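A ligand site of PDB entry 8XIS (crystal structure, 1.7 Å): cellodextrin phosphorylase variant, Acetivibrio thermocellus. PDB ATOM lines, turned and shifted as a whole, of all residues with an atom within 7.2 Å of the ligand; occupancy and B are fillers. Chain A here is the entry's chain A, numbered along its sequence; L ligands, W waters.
An oxygen (O3) of the ligand sits at hydrogen-bond distance from the side-chain carboxylate (OE2) of Glu 502, 3.1 Å away. The side-chain carboxylate of Asp 624 lies within hydrogen-bond range of an oxygen (O1) of the ligand (3.2 Å).
The backbone carbonyl oxygen (O) of Arg 486 sits at hydrogen-bond distance from the side-chain amide nitrogen (NE2) of Gln 492 (3.2 Å). The guanidinium group (NE) of Arg 486 is in salt-bridge range of the side-chain carboxylate (OE2) of Glu 502 (3.9 Å). The guanidinium group of Arg 501 lies within salt-bridge range of the side-chain carboxylate of Asp 624.
Residues that only touch the ligand: Arg 486 (3.98 Å) and Trp 622 (3.6 Å). Within 4 Å of the ligand: Arg 486, Glu 502, Trp 622 and Asp 624. The nearest printed residue that does not touch the ligand is Gln 874 (4.1 Å).
Water W2 lies within hydrogen-bond range of NE1 of Trp 622, NE2 of Gln 504 and O4 of the ligand. Water W1 lies within hydrogen-bond range of NE2 of Gln 874 (2.7 Å), O of Leu 888 (2.8 Å) and O2 of the ligand (3.5 Å).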
ATOM      1  N   ARG A 486      20.548   0.082  19.763  1.00  0.00           N
ATOM      2  CA  ARG A 486      20.855  -1.309  20.050  1.00  0.00           C
ATOM      3  C   ARG A 486      22.302  -1.442  20.508  1.00  0.00           C
ATOM      4  O   ARG A 486      22.965  -2.443  20.235  1.00  0.00           O
ATOM      5  CB  ARG A 486      20.613  -2.191  18.826  1.00  0.00           C
ATOM      6  CG  ARG A 486      19.241  -2.072  18.213  1.00  0.00           C
ATOM      7  CD  ARG A 486      18.133  -2.537  19.171  1.00  0.00           C
ATOM      8  NE  ARG A 486      16.811  -2.300  18.595  1.00  0.00           N
ATOM      9  CZ  ARG A 486      16.131  -1.159  18.702  1.00  0.00           C
ATOM     10  NH1 ARG A 486      16.543  -0.177  19.487  1.00  0.00           N
ATOM     11  NH2 ARG A 486      15.015  -1.007  17.994  1.00  0.00           N
ATOM     12  N   GLN A 492      25.074  -6.700  24.610  1.00  0.00           N
ATOM     13  CA  GLN A 492      25.468  -5.727  23.600  1.00  0.00           C
ATOM     14  C   GLN A 492      26.578  -4.883  24.203  1.00  0.00           C
ATOM     15  O   GLN A 492      26.330  -3.961  24.980  1.00  0.00           O
ATOM     16  CB  GLN A 492      24.265  -4.875  23.180  1.00  0.00           C
ATOM     17  CG  GLN A 492      23.045  -5.666  22.768  1.00  0.00           C
ATOM     18  CD  GLN A 492      23.221  -6.381  21.427  1.00  0.00           C
ATOM     19  OE1 GLN A 492      23.567  -7.559  21.388  1.00  0.00           O
ATOM     20  NE2 GLN A 492      22.992  -5.666  20.330  1.00  0.00           N
ATOM     21  N   ARG A 496      28.697  -0.190  18.515  1.00  0.00           N
ATOM     22  CA  ARG A 496      27.546   0.058  17.667  1.00  0.00           C
ATOM     23  C   ARG A 496      27.244   1.549  17.540  1.00  0.00           C
ATOM     24  O   ARG A 496      26.983   2.234  18.533  1.00  0.00           O
ATOM     25  CB  ARG A 496      26.334  -0.696  18.205  1.00  0.00           C
ATOM     26  CG  ARG A 496      26.385  -2.163  17.832  1.00  0.00           C
ATOM     27  CD  ARG A 496      25.172  -2.914  18.356  1.00  0.00           C
ATOM     28  NE  ARG A 496      24.796  -4.059  17.539  1.00  0.00           N
ATOM     29  CZ  ARG A 496      23.958  -3.994  16.504  1.00  0.00           C
ATOM     30  NH1 ARG A 496      23.478  -2.844  16.087  1.00  0.00           N
ATOM     31  NH2 ARG A 496      23.598  -5.122  15.896  1.00  0.00           N
ATOM     32  N   GLY A 499      21.911   3.078  14.010  1.00  0.00           N
ATOM     33  CA  GLY A 499      21.481   2.709  12.683  1.00  0.00           C
ATOM     34  C   GLY A 499      20.433   3.677  12.168  1.00  0.00           C
ATOM     35  O   GLY A 499      19.548   4.111  12.900  1.00  0.00           O
ATOM     36  N   ARG A 501      17.952   3.047  10.420  1.00  0.00           N
ATOM     37  CA  ARG A 501      16.622   2.447  10.582  1.00  0.00           C
ATOM     38  C   ARG A 501      16.219   2.235  12.039  1.00  0.00           C
ATOM     39  O   ARG A 501      15.117   1.748  12.299  1.00  0.00           O
ATOM     40  CB  ARG A 501      16.522   1.125   9.794  1.00  0.00           C
ATOM     41  CG  ARG A 501      17.166  -0.090  10.433  1.00  0.00           C
ATOM     42  CD  ARG A 501      16.818  -1.379   9.625  1.00  0.00           C
ATOM     43  NE  ARG A 501      17.350  -1.359   8.261  1.00  0.00           N
ATOM     44  CZ  ARG A 501      18.377  -2.086   7.852  1.00  0.00           C
ATOM     45  NH1 ARG A 501      19.058  -2.872   8.681  1.00  0.00           N
ATOM     46  NH2 ARG A 501      18.717  -2.073   6.549  1.00  0.00           N
ATOM     47  N   GLU A 502      17.052   2.592  13.007  1.00  0.00           N
ATOM     48  CA  GLU A 502      16.569   2.611  14.386  1.00  0.00           C
ATOM     49  C   GLU A 502      15.803   3.899  14.708  1.00  0.00           C
ATOM     50  O   GLU A 502      15.381   4.080  15.850  1.00  0.00           O
ATOM     51  CB  GLU A 502      17.716   2.414  15.374  1.00  0.00           C
ATOM     52  CG  GLU A 502      17.775   0.983  15.951  1.00  0.00           C
ATOM     53  CD  GLU A 502      18.520  -0.001  15.053  1.00  0.00           C
ATOM     54  OE1 GLU A 502      19.250   0.463  14.153  1.00  0.00           O
ATOM     55  OE2 GLU A 502      18.389  -1.225  15.250  1.00  0.00           O
ATOM     56  N   GLN A 504      13.104   4.018  13.953  1.00  0.00           N
ATOM     57  CA  GLN A 504      11.902   3.331  14.414  1.00  0.00           C
ATOM     58  C   GLN A 504      11.597   3.613  15.899  1.00  0.00           C
ATOM     59  O   GLN A 504      10.440   3.806  16.264  1.00  0.00           O
ATOM     60  CB  GLN A 504      12.039   1.827  14.216  1.00  0.00           C
ATOM     61  CG  GLN A 504      11.847   1.381  12.795  1.00  0.00           C
ATOM     62  CD  GLN A 504      12.062  -0.089  12.682  1.00  0.00           C
ATOM     63  OE1 GLN A 504      11.231  -0.884  13.143  1.00  0.00           O
ATOM     64  NE2 GLN A 504      13.189  -0.472  12.120  1.00  0.00           N
ATOM     65  N   ASP A 621      18.116  -5.087   2.307  1.00  0.00           N
ATOM     66  CA  ASP A 621      17.173  -4.086   2.795  1.00  0.00           C
ATOM     67  C   ASP A 621      17.076  -4.303   4.299  1.00  0.00           C
ATOM     68  O   ASP A 621      18.093  -4.674   4.915  1.00  0.00           O
ATOM     69  CB  ASP A 621      15.805  -4.159   2.062  1.00  0.00           C
ATOM     70  CG  ASP A 621      15.202  -5.566   1.971  1.00  0.00           C
ATOM     71  OD1 ASP A 621      15.616  -6.473   2.724  1.00  0.00           O
ATOM     72  OD2 ASP A 621      14.286  -5.759   1.090  1.00  0.00           O
ATOM     73  N   TRP A 622      15.903  -4.102   4.916  1.00  0.00           N
ATOM     74  CA  TRP A 622      15.790  -4.312   6.365  1.00  0.00           C
ATOM     75  C   TRP A 622      16.307  -5.664   6.796  1.00  0.00           C
ATOM     76  O   TRP A 622      16.748  -5.832   7.944  1.00  0.00           O
ATOM     77  CB  TRP A 622      14.322  -4.209   6.818  1.00  0.00           C
ATOM     78  CG  TRP A 622      14.045  -4.546   8.262  1.00  0.00           C
ATOM     79  CD1 TRP A 622      13.954  -3.657   9.301  1.00  0.00           C
ATOM     80  CD2 TRP A 622      13.834  -5.843   8.841  1.00  0.00           C
ATOM     81  NE1 TRP A 622      13.674  -4.323  10.463  1.00  0.00           N
ATOM     82  CE2 TRP A 622      13.620  -5.665  10.218  1.00  0.00           C
ATOM     83  CE3 TRP A 622      13.802  -7.146   8.326  1.00  0.00           C
ATOM     84  CZ2 TRP A 622      13.373  -6.718  11.080  1.00  0.00           C
ATOM     85  CZ3 TRP A 622      13.573  -8.222   9.217  1.00  0.00           C
ATOM     86  CH2 TRP A 622      13.342  -7.995  10.558  1.00  0.00           C
ATOM     87  N   ASN A 623      16.162  -6.664   5.946  1.00  0.00           N
ATOM     88  CA  ASN A 623      16.482  -8.039   6.325  1.00  0.00           C
ATOM     89  C   ASN A 623      17.971  -8.265   6.071  1.00  0.00           C
ATOM     90  O   ASN A 623      18.402  -8.376   4.920  1.00  0.00           O
ATOM     91  CB  ASN A 623      15.641  -9.049   5.543  1.00  0.00           C
ATOM     92  CG  ASN A 623      15.948 -10.475   5.944  1.00  0.00           C
ATOM     93  OD1 ASN A 623      17.062 -10.768   6.393  1.00  0.00           O
ATOM     94  ND2 ASN A 623      14.975 -11.365   5.799  1.00  0.00           N
ATOM     95  N   ASP A 624      18.730  -8.389   7.175  1.00  0.00           N
ATOM     96  CA  ASP A 624      20.174  -8.317   7.132  1.00  0.00           C
ATOM     97  C   ASP A 624      20.756  -9.318   6.151  1.00  0.00           C
ATOM     98  O   ASP A 624      21.816  -9.061   5.564  1.00  0.00           O
ATOM     99  CB  ASP A 624      20.762  -8.570   8.534  1.00  0.00           C
ATOM    100  CG  ASP A 624      20.670  -7.342   9.469  1.00  0.00           C
ATOM    101  OD1 ASP A 624      20.049  -6.325   9.112  1.00  0.00           O
ATOM    102  OD2 ASP A 624      21.260  -7.392  10.581  1.00  0.00           O
ATOM    103  N   SER A 625      20.077 -10.440   5.938  1.00  0.00           N
ATOM    104  CA  SER A 625      20.711 -11.588   5.295  1.00  0.00           C
ATOM    105  C   SER A 625      20.083 -11.955   3.951  1.00  0.00           C
ATOM    106  O   SER A 625      20.204 -13.099   3.509  1.00  0.00           O
ATOM    107  CB  SER A 625      20.708 -12.776   6.259  1.00  0.00           C
ATOM    108  OG  SER A 625      21.144 -12.384   7.562  1.00  0.00           O
ATOM    109  N   LEU A 786       9.985 -15.635  11.251  1.00  0.00           N
ATOM    110  CA  LEU A 786      10.317 -14.595  10.293  1.00  0.00           C
ATOM    111  C   LEU A 786      10.122 -15.075   8.855  1.00  0.00           C
ATOM    112  O   LEU A 786       9.686 -14.312   7.968  1.00  0.00           O
ATOM    113  CB  LEU A 786      11.791 -14.173  10.477  1.00  0.00           C
ATOM    114  CG  LEU A 786      12.270 -13.101   9.519  1.00  0.00           C
ATOM    115  CD1 LEU A 786      11.568 -11.809   9.839  1.00  0.00           C
ATOM    116  CD2 LEU A 786      13.790 -12.953   9.581  1.00  0.00           C
ATOM    117  N   GLU A 810      18.296 -16.795  12.834  1.00  0.00           N
ATOM    118  CA  GLU A 810      17.859 -16.866  11.444  1.00  0.00           C
ATOM    119  C   GLU A 810      17.429 -18.266  11.014  1.00  0.00           C
ATOM    120  O   GLU A 810      16.639 -18.380  10.059  1.00  0.00           O
ATOM    121  CB  GLU A 810      18.988 -16.359  10.511  1.00  0.00           C
ATOM    122  CG  GLU A 810      20.011 -15.348  11.150  1.00  0.00           C
ATOM    123  CD  GLU A 810      19.411 -14.057  11.757  1.00  0.00           C
ATOM    124  OE1 GLU A 810      18.454 -13.480  11.188  1.00  0.00           O
ATOM    125  OE2 GLU A 810      19.901 -13.614  12.814  1.00  0.00           O
ATOM    126  N   PHE A 815      11.559 -14.065  15.578  1.00  0.00           N
ATOM    127  CA  PHE A 815      12.161 -12.751  15.731  1.00  0.00           C
ATOM    128  C   PHE A 815      11.088 -11.810  16.225  1.00  0.00           C
ATOM    129  O   PHE A 815      10.175 -11.479  15.474  1.00  0.00           O
ATOM    130  CB  PHE A 815      12.741 -12.238  14.413  1.00  0.00           C
ATOM    131  CG  PHE A 815      14.152 -12.627  14.171  1.00  0.00           C
ATOM    132  CD1 PHE A 815      15.191 -12.013  14.860  1.00  0.00           C
ATOM    133  CD2 PHE A 815      14.460 -13.610  13.247  1.00  0.00           C
ATOM    134  CE1 PHE A 815      16.501 -12.377  14.645  1.00  0.00           C
ATOM    135  CE2 PHE A 815      15.763 -13.972  13.011  1.00  0.00           C
ATOM    136  CZ  PHE A 815      16.780 -13.363  13.708  1.00  0.00           C
ATOM    137  N   HIS A 817      10.712  -8.666  16.959  1.00  0.00           N
ATOM    138  CA  HIS A 817      10.481  -7.390  16.298  1.00  0.00           C
ATOM    139  C   HIS A 817       9.660  -7.575  15.038  1.00  0.00           C
ATOM    140  O   HIS A 817       8.631  -6.914  14.834  1.00  0.00           O
ATOM    141  CB  HIS A 817      11.832  -6.725  15.969  1.00  0.00           C
ATOM    142  CG  HIS A 817      11.732  -5.423  15.256  1.00  0.00           C
ATOM    143  ND1 HIS A 817      12.830  -4.805  14.687  1.00  0.00           N
ATOM    144  CD2 HIS A 817      10.678  -4.618  15.013  1.00  0.00           C
ATOM    145  CE1 HIS A 817      12.449  -3.671  14.134  1.00  0.00           C
ATOM    146  NE2 HIS A 817      11.139  -3.558  14.287  1.00  0.00           N
ATOM    147  N   ALA A 818      10.098  -8.510  14.179  1.00  0.00           N
ATOM    148  CA  ALA A 818       9.295  -8.879  12.999  1.00  0.00           C
ATOM    149  C   ALA A 818       7.902  -9.377  13.406  1.00  0.00           C
ATOM    150  O   ALA A 818       6.912  -9.024  12.784  1.00  0.00           O
ATOM    151  CB  ALA A 818      10.020  -9.956  12.194  1.00  0.00           C
ATOM    152  N   MET A 821       5.877  -6.349  13.955  1.00  0.00           N
ATOM    153  CA  MET A 821       5.424  -5.669  12.752  1.00  0.00           C
ATOM    154  C   MET A 821       4.265  -6.425  12.118  1.00  0.00           C
ATOM    155  O   MET A 821       3.340  -5.821  11.569  1.00  0.00           O
ATOM    156  CB  MET A 821       6.609  -5.498  11.796  1.00  0.00           C
ATOM    157  CG  MET A 821       7.656  -4.600  12.373  1.00  0.00           C
ATOM    158  SD  MET A 821       8.962  -4.108  11.264  1.00  0.00           S
ATOM    159  CE  MET A 821       9.808  -5.576  11.130  1.00  0.00           C
ATOM    160  N   GLN A 874      15.098 -10.222  22.361  1.00  0.00           N
ATOM    161  CA  GLN A 874      15.064 -10.137  20.895  1.00  0.00           C
ATOM    162  C   GLN A 874      14.300 -11.257  20.232  1.00  0.00           C
ATOM    163  O   GLN A 874      13.635 -11.017  19.220  1.00  0.00           O
ATOM    164  CB  GLN A 874      16.483 -10.136  20.326  1.00  0.00           C
ATOM    165  CG  GLN A 874      16.575 -10.161  18.843  1.00  0.00           C
ATOM    166  CD  GLN A 874      18.000 -10.239  18.341  1.00  0.00           C
ATOM    167  OE1 GLN A 874      18.584 -11.331  18.238  1.00  0.00           O
ATOM    168  NE2 GLN A 874      18.587  -9.085  18.075  1.00  0.00           N
ATOM    169  N   PRO A 886      19.574 -10.169  22.802  1.00  0.00           N
ATOM    170  CA  PRO A 886      19.704  -9.039  23.755  1.00  0.00           C
ATOM    171  C   PRO A 886      18.422  -8.393  24.217  1.00  0.00           C
ATOM    172  O   PRO A 886      17.311  -8.712  23.774  1.00  0.00           O
ATOM    173  CB  PRO A 886      20.541  -8.002  22.965  1.00  0.00           C
ATOM    174  CG  PRO A 886      20.349  -8.354  21.482  1.00  0.00           C
ATOM    175  CD  PRO A 886      19.921  -9.796  21.423  1.00  0.00           C
ATOM    176  N   LEU A 888      17.699  -5.044  24.035  1.00  0.00           N
ATOM    177  CA  LEU A 888      17.264  -3.881  23.281  1.00  0.00           C
ATOM    178  C   LEU A 888      16.766  -4.426  21.947  1.00  0.00           C
ATOM    179  O   LEU A 888      17.464  -5.195  21.280  1.00  0.00           O
ATOM    180  CB  LEU A 888      18.356  -2.855  23.039  1.00  0.00           C
ATOM    181  CG  LEU A 888      18.904  -2.099  24.268  1.00  0.00           C
ATOM    182  CD1 LEU A 888      17.859  -1.638  25.251  1.00  0.00           C
ATOM    183  CD2 LEU A 888      19.900  -3.017  24.909  1.00  0.00           C
ATOM    184  N   SER A 889      15.559  -4.017  21.565  1.00  0.00           N
ATOM    185  CA  SER A 889      14.971  -4.589  20.368  1.00  0.00           C
ATOM    186  C   SER A 889      13.763  -3.780  19.922  1.00  0.00           C
ATOM    187  O   SER A 889      13.006  -3.246  20.747  1.00  0.00           O
ATOM    188  CB  SER A 889      14.587  -6.066  20.628  1.00  0.00           C
ATOM    189  OG  SER A 889      13.624  -6.590  19.730  1.00  0.00           O
ATOM    190  N   GLY A 890      13.553  -3.731  18.603  1.00  0.00           N
ATOM    191  CA  GLY A 890      12.335  -3.142  18.096  1.00  0.00           C
ATOM    192  C   GLY A 890      11.078  -3.799  18.583  1.00  0.00           C
ATOM    193  O   GLY A 890       9.981  -3.251  18.410  1.00  0.00           O
HETATM  194  C1  LIG L   1      19.415  -5.769  14.588  1.00  0.00           C
HETATM  195  C2  LIG L   1      18.276  -5.102  13.834  1.00  0.00           C
HETATM  196  C3  LIG L   1      17.921  -5.883  12.565  1.00  0.00           C
HETATM  197  C4  LIG L   1      17.480  -7.319  12.890  1.00  0.00           C
HETATM  198  C5  LIG L   1      17.750  -8.311  11.761  1.00  0.00           C
HETATM  199  C6  LIG L   1      19.356  -7.293  14.485  1.00  0.00           C
HETATM  200  O1  LIG L   1      20.381  -7.692  13.652  1.00  0.00           O
HETATM  201  O2  LIG L   1      19.387  -5.328  15.933  1.00  0.00           O
HETATM  202  O3  LIG L   1      18.627  -3.770  13.463  1.00  0.00           O
HETATM  203  O4  LIG L   1      16.865  -5.268  11.872  1.00  0.00           O
HETATM  204  O5  LIG L   1      18.082  -7.802  14.080  1.00  0.00           O
HETATM  205  O6  LIG L   1      16.692  -9.239  11.683  1.00  0.00           O
HETATM  206  O   HOH W   1      18.435  -6.553  19.067  1.00  0.00           O
HETATM  207  O   HOH W   2      14.996  -2.728  12.453  1.00  0.00           O
